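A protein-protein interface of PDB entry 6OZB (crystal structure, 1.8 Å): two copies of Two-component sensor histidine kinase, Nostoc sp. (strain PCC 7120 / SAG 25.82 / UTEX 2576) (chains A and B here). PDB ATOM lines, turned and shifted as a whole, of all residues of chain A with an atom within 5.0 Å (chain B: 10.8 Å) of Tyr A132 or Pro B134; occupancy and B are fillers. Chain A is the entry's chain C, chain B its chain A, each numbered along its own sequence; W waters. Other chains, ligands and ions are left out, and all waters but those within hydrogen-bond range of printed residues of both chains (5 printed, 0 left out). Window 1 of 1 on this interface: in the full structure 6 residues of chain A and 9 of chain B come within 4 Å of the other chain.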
ATOM      1  N   ILE A 104     -20.635 -20.900  -3.880  1.00  0.00           N
ATOM      2  CA  ILE A 104     -20.395 -19.558  -3.372  1.00  0.00           C
ATOM      3  C   ILE A 104     -20.834 -18.540  -4.423  1.00  0.00           C
ATOM      4  O   ILE A 104     -20.228 -18.486  -5.473  1.00  0.00           O
ATOM      5  CB  ILE A 104     -18.899 -19.326  -3.079  1.00  0.00           C
ATOM      6  CG1 ILE A 104     -18.356 -20.330  -2.055  1.00  0.00           C
ATOM      7  CG2 ILE A 104     -18.646 -17.887  -2.663  1.00  0.00           C
ATOM      8  CD1 ILE A 104     -16.835 -20.519  -2.134  1.00  0.00           C
ATOM      9  N   ASP A 106     -21.056 -14.647  -5.483  1.00  0.00           N
ATOM     10  CA  ASP A 106     -20.487 -13.348  -5.223  1.00  0.00           C
ATOM     11  C   ASP A 106     -21.225 -12.350  -6.107  1.00  0.00           C
ATOM     12  O   ASP A 106     -20.967 -12.228  -7.314  1.00  0.00           O
ATOM     13  CB  ASP A 106     -18.995 -13.375  -5.493  1.00  0.00           C
ATOM     14  CG  ASP A 106     -18.308 -12.098  -5.067  1.00  0.00           C
ATOM     15  OD1 ASP A 106     -17.898 -12.013  -3.887  1.00  0.00           O
ATOM     16  OD2 ASP A 106     -18.155 -11.199  -5.925  1.00  0.00           O
ATOM     17  N   THR A 109     -19.317  -9.506  -8.322  1.00  0.00           N
ATOM     18  CA  THR A 109     -18.639  -9.918  -9.562  1.00  0.00           C
ATOM     19  C   THR A 109     -19.560 -10.670 -10.523  1.00  0.00           C
ATOM     20  O   THR A 109     -19.190 -10.925 -11.680  1.00  0.00           O
ATOM     21  CB  THR A 109     -17.427 -10.823  -9.287  1.00  0.00           C
ATOM     22  OG1 THR A 109     -17.846 -12.019  -8.604  1.00  0.00           O
ATOM     23  CG2 THR A 109     -16.379 -10.082  -8.508  1.00  0.00           C
ATOM     24  N   MET A 111     -20.411 -13.785 -10.161  1.00  0.00           N
ATOM     25  CA  MET A 111     -19.820 -15.108 -10.321  1.00  0.00           C
ATOM     26  C   MET A 111     -20.295 -16.082  -9.238  1.00  0.00           C
ATOM     27  O   MET A 111     -20.609 -15.688  -8.117  1.00  0.00           O
ATOM     28  CB  MET A 111     -18.299 -15.033 -10.293  1.00  0.00           C
ATOM     29  CG  MET A 111     -17.695 -14.021 -11.254  1.00  0.00           C
ATOM     30  SD  MET A 111     -17.864 -14.466 -13.008  1.00  0.00           S
ATOM     31  CE  MET A 111     -16.637 -15.778 -13.185  1.00  0.00           C
ATOM     32  N   ILE A 112     -20.319 -17.362  -9.592  1.00  0.00           N
ATOM     33  CA  ILE A 112     -20.624 -18.424  -8.622  1.00  0.00           C
ATOM     34  C   ILE A 112     -19.462 -19.401  -8.671  1.00  0.00           C
ATOM     35  O   ILE A 112     -18.979 -19.743  -9.749  1.00  0.00           O
ATOM     36  CB  ILE A 112     -21.952 -19.144  -8.937  1.00  0.00           C
ATOM     37  CG1 ILE A 112     -22.177 -20.291  -7.937  1.00  0.00           C
ATOM     38  CG2 ILE A 112     -21.954 -19.702 -10.357  1.00  0.00           C
ATOM     39  CD1 ILE A 112     -23.593 -20.953  -8.054  1.00  0.00           C
ATOM     40  N   GLY A 113     -18.984 -19.805  -7.502  1.00  0.00           N
ATOM     41  CA  GLY A 113     -17.883 -20.724  -7.395  1.00  0.00           C
ATOM     42  C   GLY A 113     -18.401 -22.043  -6.893  1.00  0.00           C
ATOM     43  O   GLY A 113     -19.118 -22.081  -5.891  1.00  0.00           O
ATOM     44  N   ILE A 130     -12.091 -24.665  -6.024  1.00  0.00           N
ATOM     45  CA  ILE A 130     -13.284 -23.890  -6.328  1.00  0.00           C
ATOM     46  C   ILE A 130     -13.076 -23.194  -7.656  1.00  0.00           C
ATOM     47  O   ILE A 130     -12.092 -22.485  -7.843  1.00  0.00           O
ATOM     48  CB  ILE A 130     -13.591 -22.849  -5.252  1.00  0.00           C
ATOM     49  CG1 ILE A 130     -13.730 -23.523  -3.890  1.00  0.00           C
ATOM     50  CG2 ILE A 130     -14.876 -22.106  -5.596  1.00  0.00           C
ATOM     51  CD1 ILE A 130     -13.663 -22.562  -2.730  1.00  0.00           C
ATOM     52  N   CYS A 131     -14.017 -23.424  -8.575  1.00  0.00           N
ATOM     53  CA  CYS A 131     -13.981 -22.890  -9.942  1.00  0.00           C
ATOM     54  C   CYS A 131     -15.124 -21.881 -10.142  1.00  0.00           C
ATOM     55  O   CYS A 131     -16.295 -22.209  -9.889  1.00  0.00           O
ATOM     56  CB  CYS A 131     -14.077 -24.038 -10.952  1.00  0.00           C
ATOM     57  SG  CYS A 131     -14.036 -23.555 -12.703  1.00  0.00           S
ATOM     58  N   TYR A 132     -14.800 -20.660 -10.574  1.00  0.00           N
ATOM     59  CA  TYR A 132     -15.816 -19.618 -10.707  1.00  0.00           C
ATOM     60  C   TYR A 132     -16.282 -19.419 -12.165  1.00  0.00           C
ATOM     61  O   TYR A 132     -15.494 -19.420 -13.096  1.00  0.00           O
ATOM     62  CB  TYR A 132     -15.304 -18.270 -10.148  1.00  0.00           C
ATOM     63  CG  TYR A 132     -15.263 -18.236  -8.625  1.00  0.00           C
ATOM     64  CD1 TYR A 132     -14.170 -18.750  -7.928  1.00  0.00           C
ATOM     65  CD2 TYR A 132     -16.308 -17.735  -7.902  1.00  0.00           C
ATOM     66  CE1 TYR A 132     -14.147 -18.755  -6.554  1.00  0.00           C
ATOM     67  CE2 TYR A 132     -16.292 -17.737  -6.520  1.00  0.00           C
ATOM     68  CZ  TYR A 132     -15.204 -18.250  -5.857  1.00  0.00           C
ATOM     69  OH  TYR A 132     -15.192 -18.249  -4.470  1.00  0.00           O
ATOM     70  N   ARG A 133     -17.588 -19.203 -12.312  1.00  0.00           N
ATOM     71  CA  ARG A 133     -18.222 -18.984 -13.610  1.00  0.00           C
ATOM     72  C   ARG A 133     -19.327 -17.951 -13.437  1.00  0.00           C
ATOM     73  O   ARG A 133     -19.731 -17.680 -12.320  1.00  0.00           O
ATOM     74  CB  ARG A 133     -18.806 -20.290 -14.156  1.00  0.00           C
ATOM     75  CG  ARG A 133     -19.892 -20.891 -13.257  1.00  0.00           C
ATOM     76  CD  ARG A 133     -20.629 -22.052 -13.933  1.00  0.00           C
ATOM     77  NE  ARG A 133     -21.572 -22.694 -12.999  1.00  0.00           N
ATOM     78  CZ  ARG A 133     -22.800 -22.246 -12.708  1.00  0.00           C
ATOM     79  NH1 ARG A 133     -23.268 -21.138 -13.264  1.00  0.00           N
ATOM     80  NH2 ARG A 133     -23.574 -22.915 -11.848  1.00  0.00           N
ATOM     81  N   PRO A 134     -19.843 -17.397 -14.540  1.00  0.00           N
ATOM     82  CA  PRO A 134     -20.954 -16.446 -14.382  1.00  0.00           C
ATOM     83  C   PRO A 134     -22.189 -17.141 -13.813  1.00  0.00           C
ATOM     84  O   PRO A 134     -22.514 -18.258 -14.215  1.00  0.00           O
ATOM     85  CB  PRO A 134     -21.202 -15.949 -15.819  1.00  0.00           C
ATOM     86  CG  PRO A 134     -19.900 -16.195 -16.525  1.00  0.00           C
ATOM     87  CD  PRO A 134     -19.401 -17.493 -15.936  1.00  0.00           C
ATOM     88  N   THR A 175     -15.163 -12.611   0.715  1.00  0.00           N
ATOM     89  CA  THR A 175     -14.469 -13.716   0.053  1.00  0.00           C
ATOM     90  C   THR A 175     -14.678 -14.968   0.869  1.00  0.00           C
ATOM     91  O   THR A 175     -14.792 -14.903   2.086  1.00  0.00           O
ATOM     92  CB  THR A 175     -12.973 -13.461  -0.095  1.00  0.00           C
ATOM     93  OG1 THR A 175     -12.416 -13.283   1.202  1.00  0.00           O
ATOM     94  CG2 THR A 175     -12.712 -12.232  -0.951  1.00  0.00           C
ATOM     95  N   VAL A 176     -14.705 -16.116   0.206  1.00  0.00           N
ATOM     96  CA  VAL A 176     -14.898 -17.367   0.898  1.00  0.00           C
ATOM     97  C   VAL A 176     -13.767 -18.299   0.546  1.00  0.00           C
ATOM     98  O   VAL A 176     -13.481 -18.539  -0.625  1.00  0.00           O
ATOM     99  CB  VAL A 176     -16.279 -18.007   0.540  1.00  0.00           C
ATOM    100  CG1 VAL A 176     -16.452 -19.352   1.240  1.00  0.00           C
ATOM    101  CG2 VAL A 176     -17.402 -17.071   0.879  1.00  0.00           C
ATOM    102  N   GLN B  91      -3.072 -15.315   5.043  1.00  0.00           N
ATOM    103  CA  GLN B  91      -3.496 -16.188   3.943  1.00  0.00           C
ATOM    104  C   GLN B  91      -2.706 -15.878   2.667  1.00  0.00           C
ATOM    105  O   GLN B  91      -2.135 -16.761   2.038  1.00  0.00           O
ATOM    106  CB  GLN B  91      -4.992 -16.001   3.670  1.00  0.00           C
ATOM    107  CG  GLN B  91      -5.941 -16.712   4.624  1.00  0.00           C
ATOM    108  CD  GLN B  91      -7.399 -16.648   4.159  1.00  0.00           C
ATOM    109  OE1 GLN B  91      -7.769 -15.803   3.338  1.00  0.00           O
ATOM    110  NE2 GLN B  91      -8.231 -17.536   4.693  1.00  0.00           N
ATOM    111  N   LEU B  95       0.480 -18.139   0.645  1.00  0.00           N
ATOM    112  CA  LEU B  95       0.492 -18.481  -0.768  1.00  0.00           C
ATOM    113  C   LEU B  95       1.821 -18.082  -1.403  1.00  0.00           C
ATOM    114  O   LEU B  95       2.368 -18.818  -2.218  1.00  0.00           O
ATOM    115  CB  LEU B  95      -0.659 -17.775  -1.506  1.00  0.00           C
ATOM    116  CG  LEU B  95      -2.088 -18.210  -1.203  1.00  0.00           C
ATOM    117  CD1 LEU B  95      -3.108 -17.399  -2.026  1.00  0.00           C
ATOM    118  CD2 LEU B  95      -2.218 -19.700  -1.453  1.00  0.00           C
ATOM    119  N   SER B 103       0.217 -13.472  -8.836  1.00  0.00           N
ATOM    120  CA  SER B 103      -1.139 -12.933  -8.725  1.00  0.00           C
ATOM    121  C   SER B 103      -1.393 -11.793  -9.688  1.00  0.00           C
ATOM    122  O   SER B 103      -0.606 -10.846  -9.786  1.00  0.00           O
ATOM    123  CB  SER B 103      -1.416 -12.432  -7.305  1.00  0.00           C
ATOM    124  OG  SER B 103      -1.385 -13.487  -6.370  1.00  0.00           O
ATOM    125  N   ILE B 104      -2.541 -11.889 -10.363  1.00  0.00           N
ATOM    126  CA  ILE B 104      -3.017 -10.908 -11.303  1.00  0.00           C
ATOM    127  C   ILE B 104      -4.345 -10.341 -10.809  1.00  0.00           C
ATOM    128  O   ILE B 104      -5.328 -11.088 -10.753  1.00  0.00           O
ATOM    129  CB  ILE B 104      -3.263 -11.544 -12.692  1.00  0.00           C
ATOM    130  CG1 ILE B 104      -1.982 -12.158 -13.293  1.00  0.00           C
ATOM    131  CG2 ILE B 104      -3.874 -10.537 -13.625  1.00  0.00           C
ATOM    132  CD1 ILE B 104      -2.230 -13.178 -14.377  1.00  0.00           C
ATOM    133  N   VAL B 105      -4.390  -9.057 -10.457  1.00  0.00           N
ATOM    134  CA  VAL B 105      -5.652  -8.414 -10.065  1.00  0.00           C
ATOM    135  C   VAL B 105      -6.195  -7.574 -11.200  1.00  0.00           C
ATOM    136  O   VAL B 105      -5.461  -6.756 -11.804  1.00  0.00           O
ATOM    137  CB  VAL B 105      -5.505  -7.529  -8.802  1.00  0.00           C
ATOM    138  CG1 VAL B 105      -6.843  -6.945  -8.400  1.00  0.00           C
ATOM    139  CG2 VAL B 105      -4.969  -8.331  -7.636  1.00  0.00           C
ATOM    140  N   ASP B 106      -7.472  -7.824 -11.512  1.00  0.00           N
ATOM    141  CA  ASP B 106      -8.219  -7.114 -12.541  1.00  0.00           C
ATOM    142  C   ASP B 106      -9.345  -6.324 -11.893  1.00  0.00           C
ATOM    143  O   ASP B 106     -10.380  -6.877 -11.506  1.00  0.00           O
ATOM    144  CB  ASP B 106      -8.772  -8.095 -13.573  1.00  0.00           C
ATOM    145  CG  ASP B 106      -9.377  -7.403 -14.799  1.00  0.00           C
ATOM    146  OD1 ASP B 106      -8.623  -7.097 -15.753  1.00  0.00           O
ATOM    147  OD2 ASP B 106     -10.613  -7.225 -14.836  1.00  0.00           O
ATOM    148  N   VAL B 107      -9.138  -5.019 -11.753  1.00  0.00           N
ATOM    149  CA  VAL B 107     -10.079  -4.191 -11.057  1.00  0.00           C
ATOM    150  C   VAL B 107     -11.424  -4.155 -11.768  1.00  0.00           C
ATOM    151  O   VAL B 107     -12.463  -4.213 -11.103  1.00  0.00           O
ATOM    152  CB  VAL B 107      -9.513  -2.787 -10.883  1.00  0.00           C
ATOM    153  CG1 VAL B 107     -10.587  -1.835 -10.361  1.00  0.00           C
ATOM    154  CG2 VAL B 107      -8.336  -2.849  -9.911  1.00  0.00           C
ATOM    155  N   ALA B 108     -11.434  -4.076 -13.098  1.00  0.00           N
ATOM    156  CA  ALA B 108     -12.703  -3.965 -13.815  1.00  0.00           C
ATOM    157  C   ALA B 108     -13.672  -5.119 -13.545  1.00  0.00           C
ATOM    158  O   ALA B 108     -14.881  -4.899 -13.408  1.00  0.00           O
ATOM    159  CB  ALA B 108     -12.464  -3.849 -15.325  1.00  0.00           C
ATOM    160  N   THR B 109     -13.152  -6.331 -13.443  1.00  0.00           N
ATOM    161  CA  THR B 109     -13.980  -7.513 -13.190  1.00  0.00           C
ATOM    162  C   THR B 109     -14.054  -7.878 -11.703  1.00  0.00           C
ATOM    163  O   THR B 109     -14.862  -8.725 -11.317  1.00  0.00           O
ATOM    164  CB  THR B 109     -13.461  -8.765 -13.933  1.00  0.00           C
ATOM    165  OG1 THR B 109     -12.117  -9.061 -13.528  1.00  0.00           O
ATOM    166  CG2 THR B 109     -13.508  -8.587 -15.454  1.00  0.00           C
ATOM    167  N   GLY B 110     -13.190  -7.276 -10.891  1.00  0.00           N
ATOM    168  CA  GLY B 110     -13.147  -7.584  -9.470  1.00  0.00           C
ATOM    169  C   GLY B 110     -12.583  -8.962  -9.165  1.00  0.00           C
ATOM    170  O   GLY B 110     -12.894  -9.562  -8.118  1.00  0.00           O
ATOM    171  N   MET B 111     -11.742  -9.462 -10.070  1.00  0.00           N
ATOM    172  CA  MET B 111     -11.180 -10.796  -9.942  1.00  0.00           C
ATOM    173  C   MET B 111      -9.661 -10.795  -9.742  1.00  0.00           C
ATOM    174  O   MET B 111      -8.950  -9.879 -10.165  1.00  0.00           O
ATOM    175  CB  MET B 111     -11.509 -11.634 -11.178  1.00  0.00           C
ATOM    176  CG  MET B 111     -12.954 -11.643 -11.559  1.00  0.00           C
ATOM    177  SD  MET B 111     -14.071 -12.508 -10.421  1.00  0.00           S
ATOM    178  CE  MET B 111     -13.641 -14.212 -10.761  1.00  0.00           C
ATOM    179  N   ILE B 112      -9.185 -11.840  -9.077  1.00  0.00           N
ATOM    180  CA  ILE B 112      -7.755 -12.074  -8.942  1.00  0.00           C
ATOM    181  C   ILE B 112      -7.445 -13.446  -9.467  1.00  0.00           C
ATOM    182  O   ILE B 112      -8.142 -14.409  -9.167  1.00  0.00           O
ATOM    183  CB  ILE B 112      -7.291 -11.926  -7.465  1.00  0.00           C
ATOM    184  CG1 ILE B 112      -5.774 -12.191  -7.349  1.00  0.00           C
ATOM    185  CG2 ILE B 112      -8.084 -12.826  -6.572  1.00  0.00           C
ATOM    186  CD1 ILE B 112      -5.133 -11.830  -5.987  1.00  0.00           C
ATOM    187  N   GLY B 113      -6.412 -13.528 -10.295  1.00  0.00           N
ATOM    188  CA  GLY B 113      -6.008 -14.790 -10.857  1.00  0.00           C
ATOM    189  C   GLY B 113      -4.695 -15.219 -10.246  1.00  0.00           C
ATOM    190  O   GLY B 113      -3.789 -14.407 -10.120  1.00  0.00           O
ATOM    191  N   GLN B 114      -4.593 -16.485  -9.874  1.00  0.00           N
ATOM    192  CA  GLN B 114      -3.420 -16.949  -9.170  1.00  0.00           C
ATOM    193  C   GLN B 114      -2.879 -18.180  -9.842  1.00  0.00           C
ATOM    194  O   GLN B 114      -3.624 -19.070 -10.271  1.00  0.00           O
ATOM    195  CB  GLN B 114      -3.752 -17.164  -7.702  1.00  0.00           C
ATOM    196  CG  GLN B 114      -3.896 -15.788  -7.012  1.00  0.00           C
ATOM    197  CD  GLN B 114      -4.054 -15.852  -5.524  1.00  0.00           C
ATOM    198  OE1 GLN B 114      -4.806 -16.664  -5.008  1.00  0.00           O
ATOM    199  NE2 GLN B 114      -3.376 -14.949  -4.820  1.00  0.00           N
ATOM    200  N   ASP B 129      -3.153 -23.996 -15.155  1.00  0.00           N
ATOM    201  CA  ASP B 129      -3.196 -22.599 -15.552  1.00  0.00           C
ATOM    202  C   ASP B 129      -3.612 -21.601 -14.453  1.00  0.00           C
ATOM    203  O   ASP B 129      -3.485 -21.869 -13.255  1.00  0.00           O
ATOM    204  CB  ASP B 129      -4.147 -22.496 -16.755  1.00  0.00           C
ATOM    205  CG  ASP B 129      -5.464 -23.230 -16.527  1.00  0.00           C
ATOM    206  OD1 ASP B 129      -5.957 -23.234 -15.379  1.00  0.00           O
ATOM    207  OD2 ASP B 129      -6.003 -23.807 -17.496  1.00  0.00           O
ATOM    208  N   ILE B 130      -4.028 -20.416 -14.890  1.00  0.00           N
ATOM    209  CA  ILE B 130      -4.411 -19.329 -14.008  1.00  0.00           C
ATOM    210  C   ILE B 130      -5.905 -19.398 -13.679  1.00  0.00           C
ATOM    211  O   ILE B 130      -6.779 -19.346 -14.575  1.00  0.00           O
ATOM    212  CB  ILE B 130      -4.061 -17.995 -14.654  1.00  0.00           C
ATOM    213  CG1 ILE B 130      -2.576 -18.005 -15.079  1.00  0.00           C
ATOM    214  CG2 ILE B 130      -4.372 -16.839 -13.710  1.00  0.00           C
ATOM    215  CD1 ILE B 130      -2.189 -16.905 -16.059  1.00  0.00           C
ATOM    216  N   CYS B 131      -6.202 -19.442 -12.385  1.00  0.00           N
ATOM    217  CA  CYS B 131      -7.572 -19.623 -11.914  1.00  0.00           C
ATOM    218  C   CYS B 131      -8.017 -18.324 -11.255  1.00  0.00           C
ATOM    219  O   CYS B 131      -7.323 -17.801 -10.371  1.00  0.00           O
ATOM    220  CB  CYS B 131      -7.649 -20.809 -10.942  1.00  0.00           C
ATOM    221  SG  CYS B 131      -9.295 -21.215 -10.326  1.00  0.00           S
ATOM    222  N   TYR B 132      -9.129 -17.770 -11.732  1.00  0.00           N
ATOM    223  CA  TYR B 132      -9.622 -16.484 -11.243  1.00  0.00           C
ATOM    224  C   TYR B 132     -10.776 -16.648 -10.246  1.00  0.00           C
ATOM    225  O   TYR B 132     -11.682 -17.447 -10.447  1.00  0.00           O
ATOM    226  CB  TYR B 132     -10.082 -15.594 -12.427  1.00  0.00           C
ATOM    227  CG  TYR B 132      -8.922 -15.000 -13.210  1.00  0.00           C
ATOM    228  CD1 TYR B 132      -8.300 -15.723 -14.212  1.00  0.00           C
ATOM    229  CD2 TYR B 132      -8.453 -13.726 -12.936  1.00  0.00           C
ATOM    230  CE1 TYR B 132      -7.222 -15.191 -14.914  1.00  0.00           C
ATOM    231  CE2 TYR B 132      -7.384 -13.184 -13.636  1.00  0.00           C
ATOM    232  CZ  TYR B 132      -6.776 -13.923 -14.615  1.00  0.00           C
ATOM    233  OH  TYR B 132      -5.716 -13.373 -15.285  1.00  0.00           O
ATOM    234  N   ARG B 133     -10.740 -15.819  -9.200  1.00  0.00           N
ATOM    235  CA  ARG B 133     -11.763 -15.789  -8.148  1.00  0.00           C
ATOM    236  C   ARG B 133     -11.997 -14.340  -7.733  1.00  0.00           C
ATOM    237  O   ARG B 133     -11.238 -13.460  -8.090  1.00  0.00           O
ATOM    238  CB  ARG B 133     -11.324 -16.602  -6.933  1.00  0.00           C
ATOM    239  CG  ARG B 133     -10.035 -16.054  -6.300  1.00  0.00           C
ATOM    240  CD  ARG B 133      -9.741 -16.709  -4.966  1.00  0.00           C
ATOM    241  NE  ARG B 133      -8.419 -16.321  -4.433  1.00  0.00           N
ATOM    242  CZ  ARG B 133      -8.175 -15.194  -3.767  1.00  0.00           C
ATOM    243  NH1 ARG B 133      -9.147 -14.317  -3.564  1.00  0.00           N
ATOM    244  NH2 ARG B 133      -6.952 -14.932  -3.306  1.00  0.00           N
ATOM    245  N   PRO B 134     -13.070 -14.080  -6.988  1.00  0.00           N
ATOM    246  CA  PRO B 134     -13.281 -12.695  -6.549  1.00  0.00           C
ATOM    247  C   PRO B 134     -12.196 -12.238  -5.598  1.00  0.00           C
ATOM    248  O   PRO B 134     -11.788 -13.017  -4.730  1.00  0.00           O
ATOM    249  CB  PRO B 134     -14.641 -12.749  -5.875  1.00  0.00           C
ATOM    250  CG  PRO B 134     -15.320 -13.956  -6.518  1.00  0.00           C
ATOM    251  CD  PRO B 134     -14.223 -14.943  -6.679  1.00  0.00           C
ATOM    252  N   VAL B 135     -11.719 -11.009  -5.788  1.00  0.00           N
ATOM    253  CA  VAL B 135     -10.651 -10.487  -4.948  1.00  0.00           C
ATOM    254  C   VAL B 135     -11.260  -9.735  -3.766  1.00  0.00           C
ATOM    255  O   VAL B 135     -12.301  -9.116  -3.883  1.00  0.00           O
ATOM    256  CB  VAL B 135      -9.678  -9.573  -5.760  1.00  0.00           C
ATOM    257  CG1 VAL B 135     -10.366  -8.312  -6.212  1.00  0.00           C
ATOM    258  CG2 VAL B 135      -8.395  -9.253  -4.939  1.00  0.00           C
ATOM    259  N   ASP B 136     -10.626  -9.816  -2.613  1.00  0.00           N
ATOM    260  CA  ASP B 136     -11.145  -9.114  -1.434  1.00  0.00           C
ATOM    261  C   ASP B 136     -11.289  -7.618  -1.704  1.00  0.00           C
ATOM    262  O   ASP B 136     -10.411  -6.988  -2.320  1.00  0.00           O
ATOM    263  CB  ASP B 136     -10.235  -9.351  -0.237  1.00  0.00           C
ATOM    264  CG  ASP B 136     -10.906  -9.005   1.076  1.00  0.00           C
ATOM    265  OD1 ASP B 136     -11.037  -7.810   1.364  1.00  0.00           O
ATOM    266  OD2 ASP B 136     -11.324  -9.919   1.815  1.00  0.00           O
ATOM    267  N   SER B 137     -12.413  -7.047  -1.287  1.00  0.00           N
ATOM    268  CA  SER B 137     -12.685  -5.645  -1.591  1.00  0.00           C
ATOM    269  C   SER B 137     -11.679  -4.712  -0.897  1.00  0.00           C
ATOM    270  O   SER B 137     -11.438  -3.613  -1.384  1.00  0.00           O
ATOM    271  CB  SER B 137     -14.127  -5.266  -1.225  1.00  0.00           C
ATOM    272  OG  SER B 137     -14.345  -5.440   0.152  1.00  0.00           O
ATOM    273  N   CYS B 138     -11.062  -5.137   0.208  1.00  0.00           N
ATOM    274  CA  CYS B 138     -10.048  -4.281   0.833  1.00  0.00           C
ATOM    275  C   CYS B 138      -8.863  -4.057  -0.115  1.00  0.00           C
ATOM    276  O   CYS B 138      -8.305  -2.953  -0.202  1.00  0.00           O
ATOM    277  CB  CYS B 138      -9.556  -4.865   2.140  1.00  0.00           C
ATOM    278  SG  CYS B 138      -8.384  -3.781   2.967  1.00  0.00           S
ATOM    279  N   HIS B 139      -8.466  -5.128  -0.801  1.00  0.00           N
ATOM    280  CA  HIS B 139      -7.340  -5.074  -1.716  1.00  0.00           C
ATOM    281  C   HIS B 139      -7.707  -4.304  -2.962  1.00  0.00           C
ATOM    282  O   HIS B 139      -6.879  -3.577  -3.498  1.00  0.00           O
ATOM    283  CB  HIS B 139      -6.877  -6.486  -2.061  1.00  0.00           C
ATOM    284  CG  HIS B 139      -5.583  -6.555  -2.803  1.00  0.00           C
ATOM    285  ND1 HIS B 139      -4.487  -5.764  -2.503  1.00  0.00           N
ATOM    286  CD2 HIS B 139      -5.199  -7.372  -3.814  1.00  0.00           C
ATOM    287  CE1 HIS B 139      -3.491  -6.092  -3.311  1.00  0.00           C
ATOM    288  NE2 HIS B 139      -3.894  -7.061  -4.114  1.00  0.00           N
ATOM    289  N   VAL B 140      -8.944  -4.454  -3.429  1.00  0.00           N
ATOM    290  CA  VAL B 140      -9.414  -3.688  -4.578  1.00  0.00           C
ATOM    291  C   VAL B 140      -9.287  -2.211  -4.270  1.00  0.00           C
ATOM    292  O   VAL B 140      -8.799  -1.410  -5.070  1.00  0.00           O
ATOM    293  CB  VAL B 140     -10.916  -3.984  -4.906  1.00  0.00           C
ATOM    294  CG1 VAL B 140     -11.551  -2.867  -5.733  1.00  0.00           C
ATOM    295  CG2 VAL B 140     -10.993  -5.242  -5.632  1.00  0.00           C
HETATM  296  O   HOH W   1     -17.409  -9.060 -12.713  1.00  0.00           O
HETATM  297  O   HOH W   2     -13.808 -10.425   2.340  1.00  0.00           O
HETATM  298  O   HOH W   3     -10.080 -12.348   1.962  1.00  0.00           O
HETATM  299  O   HOH W   4     -12.022 -20.006 -10.930  1.00  0.00           O
HETATM  300  O   HOH W   5     -10.721 -20.070  -7.032  1.00  0.00           O
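O of Arg B133 sits at hydrogen-bond distance from N of Ile B112 (2.8 Å).
The backbone carbonyl oxygen (O) of Cys B131 is in hydrogen-bond range of the backbone NH (N) of Gln B114 (3.1 Å).
NH2 of Arg B133 is in hydrogen-bond range of OE1 of Gln B114, 3.2 Å away.
The side-chain carboxylate (OD1) of Asp B136 is in hydrogen-bond range of the backbone NH (N) of Cys B138 (2.9 Å).
The side-chain carboxylate (OD2) of Asp A106 lies within hydrogen-bond range of the side-chain hydroxyl (OG1) of Thr A109, at 2.8 Å.
The side-chain hydroxyl (OG1) of Thr A109 lies close to the backbone NH (N) of Met A111, at 3.5 Å.
Pro B134 touches Asp A106 (CG to CG, 3.8 Å).
O of Thr B109 touches CG2 of Thr A109, at 3.5 Å.
Gly B110 touches Thr A109.
Thr A109 touches Met B111.
OG1 of Thr A109 touches CG of Pro B134, 3.8 Å away.
Tyr B132 touches Tyr A132.
CE1 of Tyr A132 touches CB of Arg B133, 3.6 Å away.
CD of Pro B134 touches CE2 of Tyr A132, at 3.5 Å.
CG2 of Thr A175 touches O of Pro B134, at 3.97 Å.
CG2 of Thr A175 touches CA of Asp B136, at 3.5 Å.
Pro B134 touches just these residues of chain A: Asp A106 (3.8 Å), Thr A109 (3.8 Å), Tyr A132 (3.5 Å) and Thr A175 (3.97 Å).
No residue of chain B comes within 4 Å of Ile A104.
Of chain B, only Pro B134 comes within 4 Å of Asp A106.
No residue of chain B comes within 4 Å of Gly A113.
Printed residues of chain A within 4 Å of Tyr B132: Tyr A132.
Of the printed residues of chain A, Cys B131 touches Ile A130.
Of the printed residues of chain B, Ile A130 touches Cys B131 (3.9 Å).
Of the printed residues of chain A, Asp B136 touches Thr A175 (3.5 Å).
Printed residues of chain B within 4 Å of Thr A175: Pro B134 and Asp B136.
The nearest residue of chain A that does not touch Pro B134 is Met A111 (4.9 Å).
Of the 13 printed residues of chain A, 5 touch a printed residue of chain B.
Hydrophobic or aromatic side chains of chain A within 4 Å of the printed part of chain B: Tyr A132.
Of the 26 printed residues of chain B, 8 touch a printed residue of chain A.
Hydrophobic or aromatic side chains of chain B that line the printed part of chain A: Met B111 and Pro B134.
Thr A109 touches Met B111, but with the chains exchanged Met A111 does not touch Thr B109 (6.0 Å).
Thr A109 touches Pro B134, but with the chains exchanged Pro A134 does not touch Thr B109 (10.0 Å).
Tyr A132 touches Arg B133, but with the chains exchanged Arg A133 does not touch Tyr B132 (6.4 Å).
Tyr A132 touches Pro B134, but with the chains exchanged Pro A134 does not touch Tyr B132 (9.1 Å).
Water W2 lies within hydrogen-bond range of OD2 of Asp B136 (2.6 Å) and N of Thr A175 (3.0 Å).
Water W4 lies within hydrogen-bond range of O of Tyr B132 (2.6 Å), N of Tyr A132 (2.9 Å) and SG of Cys B131 (3.0 Å).
Water W3 bridges OG1 of Thr A175 (2.6 Å) and OD2 of Asp B136 (2.7 Å).
Water W1 bridges O of Thr A109 and O of Thr B109.
Water W5 lies within hydrogen-bond range of the backbone carbonyl oxygen of Ile A130 (2.9 Å) and the side-chain sulfur of Cys B131 (3.8 Å).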
